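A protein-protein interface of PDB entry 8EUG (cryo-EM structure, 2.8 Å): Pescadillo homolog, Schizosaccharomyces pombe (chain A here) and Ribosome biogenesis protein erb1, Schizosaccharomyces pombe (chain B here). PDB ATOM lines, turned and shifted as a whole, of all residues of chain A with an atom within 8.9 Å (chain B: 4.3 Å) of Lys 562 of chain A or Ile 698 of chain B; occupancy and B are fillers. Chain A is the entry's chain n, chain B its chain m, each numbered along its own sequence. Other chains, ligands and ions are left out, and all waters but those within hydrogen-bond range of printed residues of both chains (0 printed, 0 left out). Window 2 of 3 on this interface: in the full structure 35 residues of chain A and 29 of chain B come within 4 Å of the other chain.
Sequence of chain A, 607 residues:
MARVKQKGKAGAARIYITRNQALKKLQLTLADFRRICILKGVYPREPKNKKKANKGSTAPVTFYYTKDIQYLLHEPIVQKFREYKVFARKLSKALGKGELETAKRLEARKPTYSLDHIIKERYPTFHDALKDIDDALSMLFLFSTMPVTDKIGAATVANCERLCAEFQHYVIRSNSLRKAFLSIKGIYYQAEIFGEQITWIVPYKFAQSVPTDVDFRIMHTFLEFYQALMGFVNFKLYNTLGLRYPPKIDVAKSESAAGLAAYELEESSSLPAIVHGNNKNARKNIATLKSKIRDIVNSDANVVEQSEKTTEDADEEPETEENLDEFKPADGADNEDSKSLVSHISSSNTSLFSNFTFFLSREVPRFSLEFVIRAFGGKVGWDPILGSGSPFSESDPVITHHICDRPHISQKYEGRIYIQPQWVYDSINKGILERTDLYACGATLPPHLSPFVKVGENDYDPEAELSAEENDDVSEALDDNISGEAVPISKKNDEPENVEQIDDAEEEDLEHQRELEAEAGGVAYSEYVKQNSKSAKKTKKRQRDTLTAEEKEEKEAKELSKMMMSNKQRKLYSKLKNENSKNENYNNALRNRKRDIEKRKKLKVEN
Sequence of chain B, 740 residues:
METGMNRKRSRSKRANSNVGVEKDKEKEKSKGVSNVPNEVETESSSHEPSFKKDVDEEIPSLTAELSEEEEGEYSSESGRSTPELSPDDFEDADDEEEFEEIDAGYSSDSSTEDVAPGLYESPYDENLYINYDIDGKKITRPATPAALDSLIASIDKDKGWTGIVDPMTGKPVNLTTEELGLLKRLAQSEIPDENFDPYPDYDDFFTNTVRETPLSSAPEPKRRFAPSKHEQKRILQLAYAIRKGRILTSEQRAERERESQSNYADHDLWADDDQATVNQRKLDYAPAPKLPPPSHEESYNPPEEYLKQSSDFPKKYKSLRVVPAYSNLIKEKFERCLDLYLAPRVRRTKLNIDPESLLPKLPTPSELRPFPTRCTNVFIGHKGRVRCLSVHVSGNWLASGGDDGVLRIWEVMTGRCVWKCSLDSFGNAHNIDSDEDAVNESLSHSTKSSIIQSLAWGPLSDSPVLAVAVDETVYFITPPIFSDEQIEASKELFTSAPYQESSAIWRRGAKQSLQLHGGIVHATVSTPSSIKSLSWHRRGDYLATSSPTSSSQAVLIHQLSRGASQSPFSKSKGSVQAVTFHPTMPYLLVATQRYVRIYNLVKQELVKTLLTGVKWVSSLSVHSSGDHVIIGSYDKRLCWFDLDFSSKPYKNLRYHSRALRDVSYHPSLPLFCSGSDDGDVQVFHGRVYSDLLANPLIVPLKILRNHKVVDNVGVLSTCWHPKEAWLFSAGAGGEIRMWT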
ATOM      1  N   GLU A 556      -8.159  35.045  21.094  1.00  0.00           N
ATOM      2  CA  GLU A 556      -7.237  34.454  22.060  1.00  0.00           C
ATOM      3  C   GLU A 556      -7.888  34.281  23.425  1.00  0.00           C
ATOM      4  O   GLU A 556      -7.559  33.337  24.150  1.00  0.00           O
ATOM      5  CB  GLU A 556      -5.974  35.307  22.172  1.00  0.00           C
ATOM      6  CG  GLU A 556      -5.103  35.302  20.922  1.00  0.00           C
ATOM      7  CD  GLU A 556      -4.600  33.915  20.561  1.00  0.00           C
ATOM      8  OE1 GLU A 556      -5.333  33.169  19.878  1.00  0.00           O
ATOM      9  OE2 GLU A 556      -3.467  33.571  20.959  1.00  0.00           O
ATOM     10  N   LYS A 558     -11.081  33.533  23.867  1.00  0.00           N
ATOM     11  CA  LYS A 558     -11.947  32.367  23.743  1.00  0.00           C
ATOM     12  C   LYS A 558     -11.156  31.080  23.560  1.00  0.00           C
ATOM     13  O   LYS A 558     -11.618  30.012  23.978  1.00  0.00           O
ATOM     14  CB  LYS A 558     -12.918  32.556  22.576  1.00  0.00           C
ATOM     15  CG  LYS A 558     -13.967  31.459  22.456  1.00  0.00           C
ATOM     16  CD  LYS A 558     -14.963  31.519  23.601  1.00  0.00           C
ATOM     17  CE  LYS A 558     -16.070  30.491  23.428  1.00  0.00           C
ATOM     18  NZ  LYS A 558     -17.001  30.482  24.590  1.00  0.00           N
ATOM     19  N   GLU A 559      -9.968  31.153  22.965  1.00  0.00           N
ATOM     20  CA  GLU A 559      -9.132  29.976  22.733  1.00  0.00           C
ATOM     21  C   GLU A 559      -7.877  30.132  23.586  1.00  0.00           C
ATOM     22  O   GLU A 559      -6.842  30.619  23.126  1.00  0.00           O
ATOM     23  CB  GLU A 559      -8.799  29.807  21.242  1.00  0.00           C
ATOM     24  CG  GLU A 559      -8.078  28.509  20.909  1.00  0.00           C
ATOM     25  CD  GLU A 559      -6.574  28.675  20.810  1.00  0.00           C
ATOM     26  OE1 GLU A 559      -6.120  29.758  20.387  1.00  0.00           O
ATOM     27  OE2 GLU A 559      -5.847  27.720  21.156  1.00  0.00           O
ATOM     28  N   LEU A 560      -7.988  29.721  24.851  1.00  0.00           N
ATOM     29  CA  LEU A 560      -6.852  29.678  25.763  1.00  0.00           C
ATOM     30  C   LEU A 560      -6.920  28.417  26.621  1.00  0.00           C
ATOM     31  O   LEU A 560      -6.254  28.337  27.659  1.00  0.00           O
ATOM     32  CB  LEU A 560      -6.811  30.962  26.618  1.00  0.00           C
ATOM     33  CG  LEU A 560      -5.575  31.399  27.418  1.00  0.00           C
ATOM     34  CD1 LEU A 560      -5.453  32.908  27.348  1.00  0.00           C
ATOM     35  CD2 LEU A 560      -5.656  30.984  28.879  1.00  0.00           C
ATOM     36  N   SER A 561      -7.682  27.415  26.187  1.00  0.00           N
ATOM     37  CA  SER A 561      -7.947  26.244  27.007  1.00  0.00           C
ATOM     38  C   SER A 561      -6.720  25.347  27.116  1.00  0.00           C
ATOM     39  O   SER A 561      -6.639  24.305  26.457  1.00  0.00           O
ATOM     40  CB  SER A 561      -9.136  25.460  26.442  1.00  0.00           C
ATOM     41  OG  SER A 561      -8.907  25.074  25.099  1.00  0.00           O
ATOM     42  N   LYS A 562      -5.761  25.748  27.947  1.00  0.00           N
ATOM     43  CA  LYS A 562      -4.629  24.900  28.276  1.00  0.00           C
ATOM     44  C   LYS A 562      -5.102  23.631  28.988  1.00  0.00           C
ATOM     45  O   LYS A 562      -6.290  23.432  29.254  1.00  0.00           O
ATOM     46  CB  LYS A 562      -3.629  25.655  29.152  1.00  0.00           C
ATOM     47  CG  LYS A 562      -3.008  26.905  28.526  1.00  0.00           C
ATOM     48  CD  LYS A 562      -2.014  26.562  27.415  1.00  0.00           C
ATOM     49  CE  LYS A 562      -2.643  26.568  26.029  1.00  0.00           C
ATOM     50  NZ  LYS A 562      -1.634  26.332  24.955  1.00  0.00           N
ATOM     51  N   MET A 563      -4.143  22.765  29.305  1.00  0.00           N
ATOM     52  CA  MET A 563      -4.453  21.506  29.967  1.00  0.00           C
ATOM     53  C   MET A 563      -5.081  21.792  31.325  1.00  0.00           C
ATOM     54  O   MET A 563      -4.380  22.089  32.297  1.00  0.00           O
ATOM     55  CB  MET A 563      -3.165  20.687  30.097  1.00  0.00           C
ATOM     56  CG  MET A 563      -3.173  19.491  31.032  1.00  0.00           C
ATOM     57  SD  MET A 563      -1.614  18.607  30.808  1.00  0.00           S
ATOM     58  CE  MET A 563      -1.602  17.462  32.181  1.00  0.00           C
ATOM     59  N   MET A 564      -6.413  21.719  31.391  1.00  0.00           N
ATOM     60  CA  MET A 564      -7.140  21.983  32.631  1.00  0.00           C
ATOM     61  C   MET A 564      -8.294  21.034  32.900  1.00  0.00           C
ATOM     62  O   MET A 564      -8.755  20.979  34.045  1.00  0.00           O
ATOM     63  CB  MET A 564      -7.690  23.415  32.646  1.00  0.00           C
ATOM     64  CG  MET A 564      -6.651  24.518  32.625  1.00  0.00           C
ATOM     65  SD  MET A 564      -6.969  25.677  31.283  1.00  0.00           S
ATOM     66  CE  MET A 564      -8.372  26.570  31.954  1.00  0.00           C
ATOM     67  N   MET A 565      -8.777  20.289  31.904  1.00  0.00           N
ATOM     68  CA  MET A 565      -9.911  19.377  32.031  1.00  0.00           C
ATOM     69  C   MET A 565     -11.103  19.958  32.782  1.00  0.00           C
ATOM     70  O   MET A 565     -11.855  20.774  32.240  1.00  0.00           O
ATOM     71  CB  MET A 565      -9.460  18.093  32.721  1.00  0.00           C
ATOM     72  CG  MET A 565      -8.553  17.244  31.866  1.00  0.00           C
ATOM     73  SD  MET A 565      -9.497  15.935  31.084  1.00  0.00           S
ATOM     74  CE  MET A 565      -9.404  14.712  32.376  1.00  0.00           C
ATOM     75  N   SER A 566     -11.281  19.522  34.031  1.00  0.00           N
ATOM     76  CA  SER A 566     -12.440  19.932  34.818  1.00  0.00           C
ATOM     77  C   SER A 566     -12.467  21.436  35.052  1.00  0.00           C
ATOM     78  O   SER A 566     -13.543  22.015  35.236  1.00  0.00           O
ATOM     79  CB  SER A 566     -12.444  19.184  36.151  1.00  0.00           C
ATOM     80  OG  SER A 566     -11.314  19.539  36.927  1.00  0.00           O
ATOM     81  N   ASN A 567     -11.297  22.078  35.066  1.00  0.00           N
ATOM     82  CA  ASN A 567     -11.250  23.527  35.217  1.00  0.00           C
ATOM     83  C   ASN A 567     -11.880  24.232  34.022  1.00  0.00           C
ATOM     84  O   ASN A 567     -12.371  25.359  34.156  1.00  0.00           O
ATOM     85  CB  ASN A 567      -9.802  23.984  35.412  1.00  0.00           C
ATOM     86  CG  ASN A 567      -9.698  25.403  35.943  1.00  0.00           C
ATOM     87  OD1 ASN A 567     -10.704  26.062  36.202  1.00  0.00           O
ATOM     88  ND2 ASN A 567      -8.469  25.880  36.112  1.00  0.00           N
ATOM     89  N   LYS A 568     -11.872  23.596  32.848  1.00  0.00           N
ATOM     90  CA  LYS A 568     -12.552  24.159  31.688  1.00  0.00           C
ATOM     91  C   LYS A 568     -14.033  24.334  31.986  1.00  0.00           C
ATOM     92  O   LYS A 568     -14.768  23.350  32.132  1.00  0.00           O
ATOM     93  CB  LYS A 568     -12.363  23.281  30.448  1.00  0.00           C
ATOM     94  CG  LYS A 568     -10.925  23.138  29.976  1.00  0.00           C
ATOM     95  CD  LYS A 568     -10.858  22.311  28.700  1.00  0.00           C
ATOM     96  CE  LYS A 568      -9.427  22.118  28.224  1.00  0.00           C
ATOM     97  NZ  LYS A 568      -8.649  21.213  29.109  1.00  0.00           N
ATOM     98  N   ARG A 570     -16.335  26.167  30.063  1.00  0.00           N
ATOM     99  CA  ARG A 570     -17.031  26.718  28.909  1.00  0.00           C
ATOM    100  C   ARG A 570     -18.478  26.257  28.824  1.00  0.00           C
ATOM    101  O   ARG A 570     -19.164  26.588  27.851  1.00  0.00           O
ATOM    102  CB  ARG A 570     -16.281  26.363  27.621  1.00  0.00           C
ATOM    103  CG  ARG A 570     -16.064  24.878  27.400  1.00  0.00           C
ATOM    104  CD  ARG A 570     -15.146  24.638  26.213  1.00  0.00           C
ATOM    105  NE  ARG A 570     -13.837  25.251  26.413  1.00  0.00           N
ATOM    106  CZ  ARG A 570     -13.391  26.304  25.742  1.00  0.00           C
ATOM    107  NH1 ARG A 570     -14.119  26.886  24.803  1.00  0.00           N
ATOM    108  NH2 ARG A 570     -12.184  26.786  26.020  1.00  0.00           N
ATOM    109  N   TRP B 640       4.046  17.978  25.711  1.00  0.00           N
ATOM    110  CA  TRP B 640       5.249  18.711  26.075  1.00  0.00           C
ATOM    111  C   TRP B 640       5.869  18.033  27.289  1.00  0.00           C
ATOM    112  O   TRP B 640       5.223  17.910  28.335  1.00  0.00           O
ATOM    113  CB  TRP B 640       4.933  20.178  26.371  1.00  0.00           C
ATOM    114  CG  TRP B 640       6.132  20.964  26.800  1.00  0.00           C
ATOM    115  CD1 TRP B 640       6.817  20.851  27.975  1.00  0.00           C
ATOM    116  CD2 TRP B 640       6.824  21.949  26.027  1.00  0.00           C
ATOM    117  NE1 TRP B 640       7.876  21.724  27.991  1.00  0.00           N
ATOM    118  CE2 TRP B 640       7.904  22.408  26.805  1.00  0.00           C
ATOM    119  CE3 TRP B 640       6.627  22.498  24.758  1.00  0.00           C
ATOM    120  CZ2 TRP B 640       8.784  23.390  26.355  1.00  0.00           C
ATOM    121  CZ3 TRP B 640       7.502  23.470  24.311  1.00  0.00           C
ATOM    122  CH2 TRP B 640       8.567  23.906  25.108  1.00  0.00           C
ATOM    123  N   LYS B 651       2.696  19.139  29.857  1.00  0.00           N
ATOM    124  CA  LYS B 651       1.411  19.628  29.378  1.00  0.00           C
ATOM    125  C   LYS B 651       0.863  18.692  28.311  1.00  0.00           C
ATOM    126  O   LYS B 651       1.619  18.064  27.562  1.00  0.00           O
ATOM    127  CB  LYS B 651       1.501  21.050  28.802  1.00  0.00           C
ATOM    128  CG  LYS B 651       1.932  22.112  29.800  1.00  0.00           C
ATOM    129  CD  LYS B 651       0.801  22.467  30.761  1.00  0.00           C
ATOM    130  CE  LYS B 651      -0.230  23.372  30.107  1.00  0.00           C
ATOM    131  NZ  LYS B 651      -1.460  23.547  30.929  1.00  0.00           N
ATOM    132  N   LEU B 653      -2.130  18.776  25.173  1.00  0.00           N
ATOM    133  CA  LEU B 653      -2.954  19.661  24.360  1.00  0.00           C
ATOM    134  C   LEU B 653      -3.722  18.827  23.348  1.00  0.00           C
ATOM    135  O   LEU B 653      -3.122  18.060  22.592  1.00  0.00           O
ATOM    136  CB  LEU B 653      -2.090  20.710  23.656  1.00  0.00           C
ATOM    137  CG  LEU B 653      -1.192  21.505  24.606  1.00  0.00           C
ATOM    138  CD1 LEU B 653      -0.223  22.381  23.842  1.00  0.00           C
ATOM    139  CD2 LEU B 653      -2.044  22.348  25.540  1.00  0.00           C
ATOM    140  N   TYR B 655      -6.217  19.966  20.923  1.00  0.00           N
ATOM    141  CA  TYR B 655      -6.979  20.916  20.123  1.00  0.00           C
ATOM    142  C   TYR B 655      -7.328  20.371  18.745  1.00  0.00           C
ATOM    143  O   TYR B 655      -8.368  20.736  18.186  1.00  0.00           O
ATOM    144  CB  TYR B 655      -6.198  22.222  19.987  1.00  0.00           C
ATOM    145  CG  TYR B 655      -5.801  22.811  21.319  1.00  0.00           C
ATOM    146  CD1 TYR B 655      -6.667  22.761  22.402  1.00  0.00           C
ATOM    147  CD2 TYR B 655      -4.556  23.399  21.499  1.00  0.00           C
ATOM    148  CE1 TYR B 655      -6.310  23.286  23.621  1.00  0.00           C
ATOM    149  CE2 TYR B 655      -4.190  23.930  22.721  1.00  0.00           C
ATOM    150  CZ  TYR B 655      -5.072  23.870  23.777  1.00  0.00           C
ATOM    151  OH  TYR B 655      -4.719  24.395  24.998  1.00  0.00           O
ATOM    152  N   PHE B 672       6.882  26.599  18.019  1.00  0.00           N
ATOM    153  CA  PHE B 672       6.760  25.237  17.520  1.00  0.00           C
ATOM    154  C   PHE B 672       5.369  25.046  16.938  1.00  0.00           C
ATOM    155  O   PHE B 672       4.425  25.765  17.277  1.00  0.00           O
ATOM    156  CB  PHE B 672       7.031  24.167  18.596  1.00  0.00           C
ATOM    157  CG  PHE B 672       6.191  24.301  19.840  1.00  0.00           C
ATOM    158  CD1 PHE B 672       6.466  25.271  20.791  1.00  0.00           C
ATOM    159  CD2 PHE B 672       5.137  23.430  20.069  1.00  0.00           C
ATOM    160  CE1 PHE B 672       5.698  25.375  21.938  1.00  0.00           C
ATOM    161  CE2 PHE B 672       4.368  23.533  21.212  1.00  0.00           C
ATOM    162  CZ  PHE B 672       4.650  24.505  22.149  1.00  0.00           C
ATOM    163  N   PHE B 684       2.363  27.397  18.128  1.00  0.00           N
ATOM    164  CA  PHE B 684       2.484  27.711  19.544  1.00  0.00           C
ATOM    165  C   PHE B 684       3.764  28.494  19.792  1.00  0.00           C
ATOM    166  O   PHE B 684       4.776  28.279  19.118  1.00  0.00           O
ATOM    167  CB  PHE B 684       2.509  26.438  20.391  1.00  0.00           C
ATOM    168  CG  PHE B 684       1.177  25.763  20.527  1.00  0.00           C
ATOM    169  CD1 PHE B 684       0.014  26.503  20.612  1.00  0.00           C
ATOM    170  CD2 PHE B 684       1.092  24.384  20.570  1.00  0.00           C
ATOM    171  CE1 PHE B 684      -1.211  25.879  20.744  1.00  0.00           C
ATOM    172  CE2 PHE B 684      -0.126  23.755  20.697  1.00  0.00           C
ATOM    173  CZ  PHE B 684      -1.280  24.502  20.789  1.00  0.00           C
ATOM    174  N   HIS B 685       3.715  29.403  20.760  1.00  0.00           N
ATOM    175  CA  HIS B 685       4.904  30.090  21.243  1.00  0.00           C
ATOM    176  C   HIS B 685       5.353  29.436  22.542  1.00  0.00           C
ATOM    177  O   HIS B 685       4.654  29.522  23.558  1.00  0.00           O
ATOM    178  CB  HIS B 685       4.638  31.578  21.464  1.00  0.00           C
ATOM    179  CG  HIS B 685       5.684  32.254  22.294  1.00  0.00           C
ATOM    180  ND1 HIS B 685       7.031  32.134  22.033  1.00  0.00           N
ATOM    181  CD2 HIS B 685       5.582  33.046  23.388  1.00  0.00           C
ATOM    182  CE1 HIS B 685       7.715  32.828  22.926  1.00  0.00           C
ATOM    183  NE2 HIS B 685       6.859  33.392  23.758  1.00  0.00           N
ATOM    184  N   PRO B 696       8.433  26.332  31.463  1.00  0.00           N
ATOM    185  CA  PRO B 696       8.259  26.801  30.082  1.00  0.00           C
ATOM    186  C   PRO B 696       6.872  27.385  29.864  1.00  0.00           C
ATOM    187  O   PRO B 696       5.867  26.849  30.334  1.00  0.00           O
ATOM    188  CB  PRO B 696       8.478  25.535  29.247  1.00  0.00           C
ATOM    189  CG  PRO B 696       8.219  24.405  30.188  1.00  0.00           C
ATOM    190  CD  PRO B 696       8.693  24.885  31.525  1.00  0.00           C
ATOM    191  N   LEU B 697       6.827  28.499  29.138  1.00  0.00           N
ATOM    192  CA  LEU B 697       5.587  29.216  28.865  1.00  0.00           C
ATOM    193  C   LEU B 697       5.075  28.794  27.494  1.00  0.00           C
ATOM    194  O   LEU B 697       5.680  29.124  26.469  1.00  0.00           O
ATOM    195  CB  LEU B 697       5.806  30.726  28.929  1.00  0.00           C
ATOM    196  CG  LEU B 697       4.558  31.590  28.749  1.00  0.00           C
ATOM    197  CD1 LEU B 697       3.566  31.339  29.874  1.00  0.00           C
ATOM    198  CD2 LEU B 697       4.930  33.061  28.674  1.00  0.00           C
ATOM    199  N   ILE B 698       3.961  28.069  27.478  1.00  0.00           N
ATOM    200  CA  ILE B 698       3.350  27.579  26.249  1.00  0.00           C
ATOM    201  C   ILE B 698       2.045  28.332  26.043  1.00  0.00           C
ATOM    202  O   ILE B 698       1.154  28.291  26.900  1.00  0.00           O
ATOM    203  CB  ILE B 698       3.111  26.063  26.301  1.00  0.00           C
ATOM    204  CG1 ILE B 698       4.401  25.337  26.682  1.00  0.00           C
ATOM    205  CG2 ILE B 698       2.589  25.560  24.966  1.00  0.00           C
ATOM    206  CD1 ILE B 698       4.191  23.893  27.067  1.00  0.00           C
ATOM    207  N   VAL B 699       1.933  29.019  24.911  1.00  0.00           N
ATOM    208  CA  VAL B 699       0.745  29.808  24.598  1.00  0.00           C
ATOM    209  C   VAL B 699       0.343  29.569  23.146  1.00  0.00           C
ATOM    210  O   VAL B 699       1.216  29.392  22.283  1.00  0.00           O
ATOM    211  CB  VAL B 699       0.986  31.301  24.884  1.00  0.00           C
ATOM    212  CG1 VAL B 699       2.002  31.882  23.914  1.00  0.00           C
ATOM    213  CG2 VAL B 699      -0.313  32.078  24.801  1.00  0.00           C
ATOM    214  N   PRO B 700      -0.951  29.518  22.834  1.00  0.00           N
ATOM    215  CA  PRO B 700      -1.360  29.494  21.426  1.00  0.00           C
ATOM    216  C   PRO B 700      -1.002  30.798  20.734  1.00  0.00           C
ATOM    217  O   PRO B 700      -1.071  31.877  21.327  1.00  0.00           O
ATOM    218  CB  PRO B 700      -2.878  29.290  21.496  1.00  0.00           C
ATOM    219  CG  PRO B 700      -3.126  28.702  22.843  1.00  0.00           C
ATOM    220  CD  PRO B 700      -2.088  29.296  23.742  1.00  0.00           C
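The side-chain hydroxyl of Tyr 655 of chain B lies within hydrogen-bond range of the backbone carbonyl oxygen of Ser 561 of chain A (2.4 Å).
The backbone carbonyl oxygen (O) of Pro 700 of chain B lies close to the side-chain carboxylate (OE2) of Glu 556 of chain A (3.0 Å).
OH of Tyr 655 of chain B sits close to N of Lys 562 of chain A (3.4 Å).
The side-chain amino group (NZ) of Lys 651 of chain B sits close to the backbone NH (N) of Met 563 of chain A, 3.2 Å away.
Lys 562 of chain A touches just these residues of chain B: Lys 651 (3.5 Å), Tyr 655 (3.2 Å), Ile 698 (3.6 Å) and Pro 700 (3.2 Å).
Of chain A, only Lys 562 (3.6 Å) comes within 4 Å of Ile 698 of chain B.
Val 699 of chain B touches none of the printed residues of chain A.
Of the printed residues of chain B, Glu 556 of chain A touches Pro 700 (3.0 Å).
Printed residues of chain B within 4 Å of Met 563 of chain A: Lys 651 (3.2 Å).
Printed residues of chain B within 4 Å of Ser 561 of chain A: Tyr 655.
Trp 640 of chain B touches none of the printed residues of chain A.
Phe 672 of chain B touches none of the printed residues of chain A.
The nearest residue of chain B that does not touch Lys 562 of chain A is Leu 653 of chain B (4.05 Å).
The nearest residue of chain A that does not touch Ile 698 of chain B is Leu 560 of chain A (7.4 Å).
The nearest printed residue of chain A that does not touch Tyr 655 of chain B is Glu 559 of chain A (4.4 Å).
NZ of Lys 568 of chain A sits at hydrogen-bond distance from O of Lys 562 of chain A (3.2 Å).
The backbone carbonyl oxygen of Lys 651 of chain B sits at hydrogen-bond distance from the backbone NH of Trp 640 of chain B (3.1 Å).
SD of Met 564 of chain A lies within hydrogen-bond range of N of Lys 562 of chain A, at 3.5 Å.
Of the 12 printed residues of chain B, 4 touch a printed residue of chain A.
Hydrophobic or aromatic side chains of chain B within 4 Å of the printed part of chain A: Tyr 655 and Pro 700.
Printed residues of chain A that touch a printed residue of chain B: Glu 556, Glu 559, Ser 561, Lys 562 and Met 563.
Among the printed residues, no Asp or Glu carboxylate lies within 4 Å of a Lys or Arg side-chain nitrogen of the other chain.
Among the printed residues, pairs that only touch across the chains: Glu 559 of chain A with Pro 700 of chain B, Lys 562 of chain A with Lys 651 of chain B, Lys 562 of chain A with Ile 698 of chain B and Lys 562 of chain A with Pro 700 of chain B.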
